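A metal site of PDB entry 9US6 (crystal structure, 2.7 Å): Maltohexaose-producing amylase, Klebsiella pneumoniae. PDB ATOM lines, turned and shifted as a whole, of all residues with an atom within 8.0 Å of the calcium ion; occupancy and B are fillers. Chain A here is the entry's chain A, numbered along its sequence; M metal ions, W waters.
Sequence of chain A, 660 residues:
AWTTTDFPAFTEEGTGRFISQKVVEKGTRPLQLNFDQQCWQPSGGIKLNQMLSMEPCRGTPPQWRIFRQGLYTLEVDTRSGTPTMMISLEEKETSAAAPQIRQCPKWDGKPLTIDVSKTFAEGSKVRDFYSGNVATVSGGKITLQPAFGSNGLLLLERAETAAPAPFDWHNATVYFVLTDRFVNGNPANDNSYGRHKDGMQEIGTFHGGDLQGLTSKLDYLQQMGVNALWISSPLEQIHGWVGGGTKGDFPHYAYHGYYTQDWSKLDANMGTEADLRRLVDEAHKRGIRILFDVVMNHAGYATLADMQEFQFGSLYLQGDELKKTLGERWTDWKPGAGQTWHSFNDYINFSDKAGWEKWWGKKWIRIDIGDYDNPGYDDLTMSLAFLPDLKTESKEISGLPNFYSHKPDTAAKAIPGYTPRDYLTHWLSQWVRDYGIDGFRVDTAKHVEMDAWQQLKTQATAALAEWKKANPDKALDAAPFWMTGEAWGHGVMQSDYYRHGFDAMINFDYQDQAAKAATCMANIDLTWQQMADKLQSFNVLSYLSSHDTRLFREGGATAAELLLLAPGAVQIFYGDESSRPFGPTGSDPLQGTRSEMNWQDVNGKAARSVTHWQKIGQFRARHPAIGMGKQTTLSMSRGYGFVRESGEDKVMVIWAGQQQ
The backbone NH of Asp 210 is in hydrogen-bond range of the backbone carbonyl oxygen of Val 183, 3.0 Å away.
The side-chain carboxylate of Asp 210 is in hydrogen-bond range of the backbone NH of Gly 213.
The side-chain carboxylate of Asp 180 lies within hydrogen-bond range of the backbone NH of Gly 208, 2.8 Å away.
O of Asp 190 lies within hydrogen-bond range of ND2 of Asn 269, 3.0 Å away.
OD2 of Asp 190 is in salt-bridge range of NZ of Lys 197 (3.8 Å).
The backbone NH of Ala 188 lies within hydrogen-bond range of the side-chain amide oxygen of Asn 186.
The side-chain amide oxygen of Asn 269 lies close to the backbone carbonyl oxygen of Asn 189 (3.1 Å).
The backbone carbonyl oxygen of Asn 189 is in hydrogen-bond range of the side-chain hydroxyl of Ser 192 (3.1 Å).
Within 4 Å of the calcium ion: Asn 184, Asn 186, Asn 189, Asp 190, Gly 208 and Asp 210.
The nearest printed residue that does not touch the calcium ion is Pro 187 (4.1 Å).
Water W1 is bound to the calcium ion (2.3 Å).
The calcium ion is bound by OD2 of Asp 210.
O of Gly 208 binds the calcium ion.
The side-chain carboxylate (OD1) of Asp 190 is bound to the calcium ion (2.4 Å).
O of Asn 186 binds the calcium ion, at 2.4 Å.
The calcium ion is bound by OD1 of Asn 189, 2.5 Å away.
OD1 of Asn 184 binds the calcium ion.
The calcium ion has seven donor atoms within binding distance.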
ATOM      1  N   THR A 179      25.905   8.606 -20.832  1.00  0.00           N
ATOM      2  CA  THR A 179      25.185   8.069 -21.975  1.00  0.00           C
ATOM      3  C   THR A 179      23.680   8.147 -21.761  1.00  0.00           C
ATOM      4  O   THR A 179      22.947   8.429 -22.712  1.00  0.00           O
ATOM      5  CB  THR A 179      25.656   6.632 -22.209  1.00  0.00           C
ATOM      6  OG1 THR A 179      27.057   6.750 -22.404  1.00  0.00           O
ATOM      7  CG2 THR A 179      25.016   5.990 -23.432  1.00  0.00           C
ATOM      8  N   ASP A 180      23.209   7.899 -20.536  1.00  0.00           N
ATOM      9  CA  ASP A 180      21.783   7.840 -20.249  1.00  0.00           C
ATOM     10  C   ASP A 180      21.100   9.184 -20.488  1.00  0.00           C
ATOM     11  O   ASP A 180      19.882   9.210 -20.699  1.00  0.00           O
ATOM     12  CB  ASP A 180      21.497   7.397 -18.824  1.00  0.00           C
ATOM     13  CG  ASP A 180      20.018   7.402 -18.441  1.00  0.00           C
ATOM     14  OD1 ASP A 180      19.263   6.584 -19.017  1.00  0.00           O
ATOM     15  OD2 ASP A 180      19.615   8.249 -17.613  1.00  0.00           O
ATOM     16  N   VAL A 183      21.471  10.845 -25.777  1.00  0.00           N
ATOM     17  CA  VAL A 183      20.542  10.588 -26.874  1.00  0.00           C
ATOM     18  C   VAL A 183      19.928   9.203 -26.698  1.00  0.00           C
ATOM     19  O   VAL A 183      20.642   8.219 -26.543  1.00  0.00           O
ATOM     20  CB  VAL A 183      21.209  10.700 -28.254  1.00  0.00           C
ATOM     21  CG1 VAL A 183      20.245  10.349 -29.392  1.00  0.00           C
ATOM     22  CG2 VAL A 183      21.820  12.078 -28.496  1.00  0.00           C
ATOM     23  N   ASN A 184      18.587   9.160 -26.771  1.00  0.00           N
ATOM     24  CA  ASN A 184      17.806   7.927 -26.713  1.00  0.00           C
ATOM     25  C   ASN A 184      17.617   7.409 -28.139  1.00  0.00           C
ATOM     26  O   ASN A 184      16.697   7.832 -28.833  1.00  0.00           O
ATOM     27  CB  ASN A 184      16.479   8.175 -26.003  1.00  0.00           C
ATOM     28  CG  ASN A 184      15.733   6.913 -25.648  1.00  0.00           C
ATOM     29  OD1 ASN A 184      16.137   5.801 -26.013  1.00  0.00           O
ATOM     30  ND2 ASN A 184      14.636   7.047 -24.922  1.00  0.00           N
ATOM     31  N   GLY A 185      18.512   6.497 -28.562  1.00  0.00           N
ATOM     32  CA  GLY A 185      18.442   5.907 -29.882  1.00  0.00           C
ATOM     33  C   GLY A 185      17.306   4.890 -30.011  1.00  0.00           C
ATOM     34  O   GLY A 185      16.749   4.742 -31.099  1.00  0.00           O
ATOM     35  N   ASN A 186      16.972   4.210 -28.910  1.00  0.00           N
ATOM     36  CA  ASN A 186      15.974   3.140 -28.901  1.00  0.00           C
ATOM     37  C   ASN A 186      15.212   3.128 -27.579  1.00  0.00           C
ATOM     38  O   ASN A 186      15.736   2.654 -26.560  1.00  0.00           O
ATOM     39  CB  ASN A 186      16.627   1.791 -29.181  1.00  0.00           C
ATOM     40  CG  ASN A 186      15.623   0.663 -29.208  1.00  0.00           C
ATOM     41  OD1 ASN A 186      14.450   0.851 -28.855  1.00  0.00           O
ATOM     42  ND2 ASN A 186      16.057  -0.511 -29.629  1.00  0.00           N
ATOM     43  N   PRO A 187      13.955   3.603 -27.534  1.00  0.00           N
ATOM     44  CA  PRO A 187      13.188   3.630 -26.283  1.00  0.00           C
ATOM     45  C   PRO A 187      12.853   2.257 -25.700  1.00  0.00           C
ATOM     46  O   PRO A 187      12.506   2.162 -24.519  1.00  0.00           O
ATOM     47  CB  PRO A 187      11.924   4.395 -26.642  1.00  0.00           C
ATOM     48  CG  PRO A 187      12.210   5.043 -27.987  1.00  0.00           C
ATOM     49  CD  PRO A 187      13.214   4.178 -28.662  1.00  0.00           C
ATOM     50  N   ALA A 188      12.953   1.189 -26.500  1.00  0.00           N
ATOM     51  CA  ALA A 188      12.558  -0.145 -26.068  1.00  0.00           C
ATOM     52  C   ALA A 188      13.354  -0.618 -24.850  1.00  0.00           C
ATOM     53  O   ALA A 188      12.834  -1.396 -24.058  1.00  0.00           O
ATOM     54  CB  ALA A 188      12.705  -1.134 -27.207  1.00  0.00           C
ATOM     55  N   ASN A 189      14.607  -0.165 -24.700  1.00  0.00           N
ATOM     56  CA  ASN A 189      15.499  -0.670 -23.670  1.00  0.00           C
ATOM     57  C   ASN A 189      15.581   0.278 -22.476  1.00  0.00           C
ATOM     58  O   ASN A 189      16.457   0.143 -21.631  1.00  0.00           O
ATOM     59  CB  ASN A 189      16.875  -1.003 -24.246  1.00  0.00           C
ATOM     60  CG  ASN A 189      17.590   0.198 -24.833  1.00  0.00           C
ATOM     61  OD1 ASN A 189      17.271   1.349 -24.491  1.00  0.00           O
ATOM     62  ND2 ASN A 189      18.563  -0.035 -25.692  1.00  0.00           N
ATOM     63  N   ASP A 190      14.638   1.236 -22.381  1.00  0.00           N
ATOM     64  CA  ASP A 190      14.675   2.248 -21.333  1.00  0.00           C
ATOM     65  C   ASP A 190      14.371   1.643 -19.961  1.00  0.00           C
ATOM     66  O   ASP A 190      14.812   2.198 -18.955  1.00  0.00           O
ATOM     67  CB  ASP A 190      13.699   3.385 -21.615  1.00  0.00           C
ATOM     68  CG  ASP A 190      14.066   4.299 -22.771  1.00  0.00           C
ATOM     69  OD1 ASP A 190      15.087   4.037 -23.445  1.00  0.00           O
ATOM     70  OD2 ASP A 190      13.319   5.277 -22.997  1.00  0.00           O
ATOM     71  N   ASN A 191      13.634   0.518 -19.933  1.00  0.00           N
ATOM     72  CA  ASN A 191      13.090  -0.026 -18.698  1.00  0.00           C
ATOM     73  C   ASN A 191      13.587  -1.443 -18.447  1.00  0.00           C
ATOM     74  O   ASN A 191      12.815  -2.301 -18.017  1.00  0.00           O
ATOM     75  CB  ASN A 191      11.564   0.006 -18.729  1.00  0.00           C
ATOM     76  CG  ASN A 191      11.025   1.403 -18.848  1.00  0.00           C
ATOM     77  OD1 ASN A 191      10.366   1.738 -19.840  1.00  0.00           O
ATOM     78  ND2 ASN A 191      11.300   2.252 -17.864  1.00  0.00           N
ATOM     79  N   SER A 192      14.882  -1.690 -18.690  1.00  0.00           N
ATOM     80  CA  SER A 192      15.471  -3.005 -18.490  1.00  0.00           C
ATOM     81  C   SER A 192      15.364  -3.409 -17.020  1.00  0.00           C
ATOM     82  O   SER A 192      15.436  -2.560 -16.136  1.00  0.00           O
ATOM     83  CB  SER A 192      16.906  -3.066 -18.948  1.00  0.00           C
ATOM     84  OG  SER A 192      17.078  -2.561 -20.269  1.00  0.00           O
ATOM     85  N   LYS A 197      10.446   5.027 -14.780  1.00  0.00           N
ATOM     86  CA  LYS A 197      10.427   6.463 -14.553  1.00  0.00           C
ATOM     87  C   LYS A 197       9.671   6.738 -13.263  1.00  0.00           C
ATOM     88  O   LYS A 197       8.825   5.946 -12.852  1.00  0.00           O
ATOM     89  CB  LYS A 197       9.728   7.183 -15.708  1.00  0.00           C
ATOM     90  CG  LYS A 197      10.234   6.902 -17.128  1.00  0.00           C
ATOM     91  CD  LYS A 197      11.706   7.212 -17.351  1.00  0.00           C
ATOM     92  CE  LYS A 197      12.012   7.682 -18.750  1.00  0.00           C
ATOM     93  NZ  LYS A 197      11.879   6.633 -19.772  1.00  0.00           N
ATOM     94  N   PHE A 206      16.688   6.286 -15.015  1.00  0.00           N
ATOM     95  CA  PHE A 206      17.207   6.121 -16.364  1.00  0.00           C
ATOM     96  C   PHE A 206      16.286   6.864 -17.338  1.00  0.00           C
ATOM     97  O   PHE A 206      15.150   6.444 -17.553  1.00  0.00           O
ATOM     98  CB  PHE A 206      17.288   4.646 -16.778  1.00  0.00           C
ATOM     99  CG  PHE A 206      18.456   3.874 -16.195  1.00  0.00           C
ATOM    100  CD1 PHE A 206      18.350   3.240 -14.958  1.00  0.00           C
ATOM    101  CD2 PHE A 206      19.655   3.763 -16.891  1.00  0.00           C
ATOM    102  CE1 PHE A 206      19.423   2.527 -14.444  1.00  0.00           C
ATOM    103  CE2 PHE A 206      20.718   3.043 -16.370  1.00  0.00           C
ATOM    104  CZ  PHE A 206      20.604   2.436 -15.148  1.00  0.00           C
ATOM    105  N   HIS A 207      16.787   7.964 -17.922  1.00  0.00           N
ATOM    106  CA  HIS A 207      16.059   8.723 -18.924  1.00  0.00           C
ATOM    107  C   HIS A 207      15.956   7.939 -20.237  1.00  0.00           C
ATOM    108  O   HIS A 207      15.042   8.192 -21.011  1.00  0.00           O
ATOM    109  CB  HIS A 207      16.707  10.089 -19.182  1.00  0.00           C
ATOM    110  CG  HIS A 207      16.594  11.040 -18.043  1.00  0.00           C
ATOM    111  ND1 HIS A 207      16.848  12.392 -18.180  1.00  0.00           N
ATOM    112  CD2 HIS A 207      16.289  10.845 -16.752  1.00  0.00           C
ATOM    113  CE1 HIS A 207      16.676  12.987 -17.011  1.00  0.00           C
ATOM    114  NE2 HIS A 207      16.342  12.066 -16.125  1.00  0.00           N
ATOM    115  N   GLY A 208      16.924   7.059 -20.507  1.00  0.00           N
ATOM    116  CA  GLY A 208      16.838   6.141 -21.635  1.00  0.00           C
ATOM    117  C   GLY A 208      17.921   6.356 -22.690  1.00  0.00           C
ATOM    118  O   GLY A 208      17.906   5.675 -23.717  1.00  0.00           O
ATOM    119  N   GLY A 209      18.861   7.275 -22.458  1.00  0.00           N
ATOM    120  CA  GLY A 209      19.969   7.459 -23.393  1.00  0.00           C
ATOM    121  C   GLY A 209      20.808   6.183 -23.517  1.00  0.00           C
ATOM    122  O   GLY A 209      20.994   5.465 -22.530  1.00  0.00           O
ATOM    123  N   ASP A 210      21.312   5.916 -24.728  1.00  0.00           N
ATOM    124  CA  ASP A 210      21.931   4.633 -25.039  1.00  0.00           C
ATOM    125  C   ASP A 210      23.092   4.816 -26.024  1.00  0.00           C
ATOM    126  O   ASP A 210      23.342   5.912 -26.510  1.00  0.00           O
ATOM    127  CB  ASP A 210      20.873   3.647 -25.522  1.00  0.00           C
ATOM    128  CG  ASP A 210      19.918   4.181 -26.588  1.00  0.00           C
ATOM    129  OD1 ASP A 210      20.402   4.853 -27.533  1.00  0.00           O
ATOM    130  OD2 ASP A 210      18.710   3.899 -26.480  1.00  0.00           O
ATOM    131  N   LEU A 211      23.787   3.705 -26.316  1.00  0.00           N
ATOM    132  CA  LEU A 211      24.957   3.703 -27.180  1.00  0.00           C
ATOM    133  C   LEU A 211      24.583   4.043 -28.618  1.00  0.00           C
ATOM    134  O   LEU A 211      25.284   4.800 -29.292  1.00  0.00           O
ATOM    135  CB  LEU A 211      25.673   2.350 -27.102  1.00  0.00           C
ATOM    136  CG  LEU A 211      26.208   1.936 -25.725  1.00  0.00           C
ATOM    137  CD1 LEU A 211      26.796   0.542 -25.802  1.00  0.00           C
ATOM    138  CD2 LEU A 211      27.246   2.910 -25.168  1.00  0.00           C
ATOM    139  N   GLN A 212      23.474   3.470 -29.110  1.00  0.00           N
ATOM    140  CA  GLN A 212      23.004   3.759 -30.454  1.00  0.00           C
ATOM    141  C   GLN A 212      22.896   5.269 -30.644  1.00  0.00           C
ATOM    142  O   GLN A 212      23.449   5.815 -31.593  1.00  0.00           O
ATOM    143  CB  GLN A 212      21.643   3.102 -30.713  1.00  0.00           C
ATOM    144  CG  GLN A 212      21.092   3.390 -32.105  1.00  0.00           C
ATOM    145  CD  GLN A 212      19.752   2.734 -32.360  1.00  0.00           C
ATOM    146  OE1 GLN A 212      19.108   2.180 -31.453  1.00  0.00           O
ATOM    147  NE2 GLN A 212      19.311   2.801 -33.601  1.00  0.00           N
ATOM    148  N   GLY A 213      22.162   5.920 -29.734  1.00  0.00           N
ATOM    149  CA  GLY A 213      21.974   7.355 -29.772  1.00  0.00           C
ATOM    150  C   GLY A 213      23.302   8.105 -29.800  1.00  0.00           C
ATOM    151  O   GLY A 213      23.484   9.019 -30.603  1.00  0.00           O
ATOM    152  N   ALA A 268      21.666  -3.674 -20.116  1.00  0.00           N
ATOM    153  CA  ALA A 268      20.695  -3.777 -21.199  1.00  0.00           C
ATOM    154  C   ALA A 268      20.163  -2.398 -21.610  1.00  0.00           C
ATOM    155  O   ALA A 268      19.745  -2.238 -22.757  1.00  0.00           O
ATOM    156  CB  ALA A 268      19.577  -4.702 -20.786  1.00  0.00           C
ATOM    157  N   ASN A 269      20.160  -1.421 -20.698  1.00  0.00           N
ATOM    158  CA  ASN A 269      19.724  -0.062 -21.016  1.00  0.00           C
ATOM    159  C   ASN A 269      20.594   0.549 -22.107  1.00  0.00           C
ATOM    160  O   ASN A 269      20.116   1.379 -22.875  1.00  0.00           O
ATOM    161  CB  ASN A 269      19.702   0.869 -19.805  1.00  0.00           C
ATOM    162  CG  ASN A 269      18.340   0.983 -19.161  1.00  0.00           C
ATOM    163  OD1 ASN A 269      17.748  -0.031 -18.771  1.00  0.00           O
ATOM    164  ND2 ASN A 269      17.833   2.197 -19.021  1.00  0.00           N
ATOM    165  N   MET A 270      21.863   0.145 -22.151  1.00  0.00           N
ATOM    166  CA  MET A 270      22.852   0.759 -23.037  1.00  0.00           C
ATOM    167  C   MET A 270      22.752   0.205 -24.454  1.00  0.00           C
ATOM    168  O   MET A 270      22.926   0.948 -25.415  1.00  0.00           O
ATOM    169  CB  MET A 270      24.273   0.511 -22.496  1.00  0.00           C
ATOM    170  CG  MET A 270      24.539   1.232 -21.190  1.00  0.00           C
ATOM    171  SD  MET A 270      24.629   3.006 -21.466  1.00  0.00           S
ATOM    172  CE  MET A 270      23.599   3.568 -20.092  1.00  0.00           C
ATOM    173  N   GLY A 271      22.485  -1.107 -24.555  1.00  0.00           N
ATOM    174  CA  GLY A 271      22.318  -1.759 -25.834  1.00  0.00           C
ATOM    175  C   GLY A 271      23.026  -3.108 -25.864  1.00  0.00           C
ATOM    176  O   GLY A 271      23.331  -3.680 -24.819  1.00  0.00           O
HETATM  177 CA    CA M   1      17.037   3.768 -24.814  1.00  0.00          CA
HETATM  178  O   HOH W   1      18.036   3.254 -22.809  1.00  0.00           O
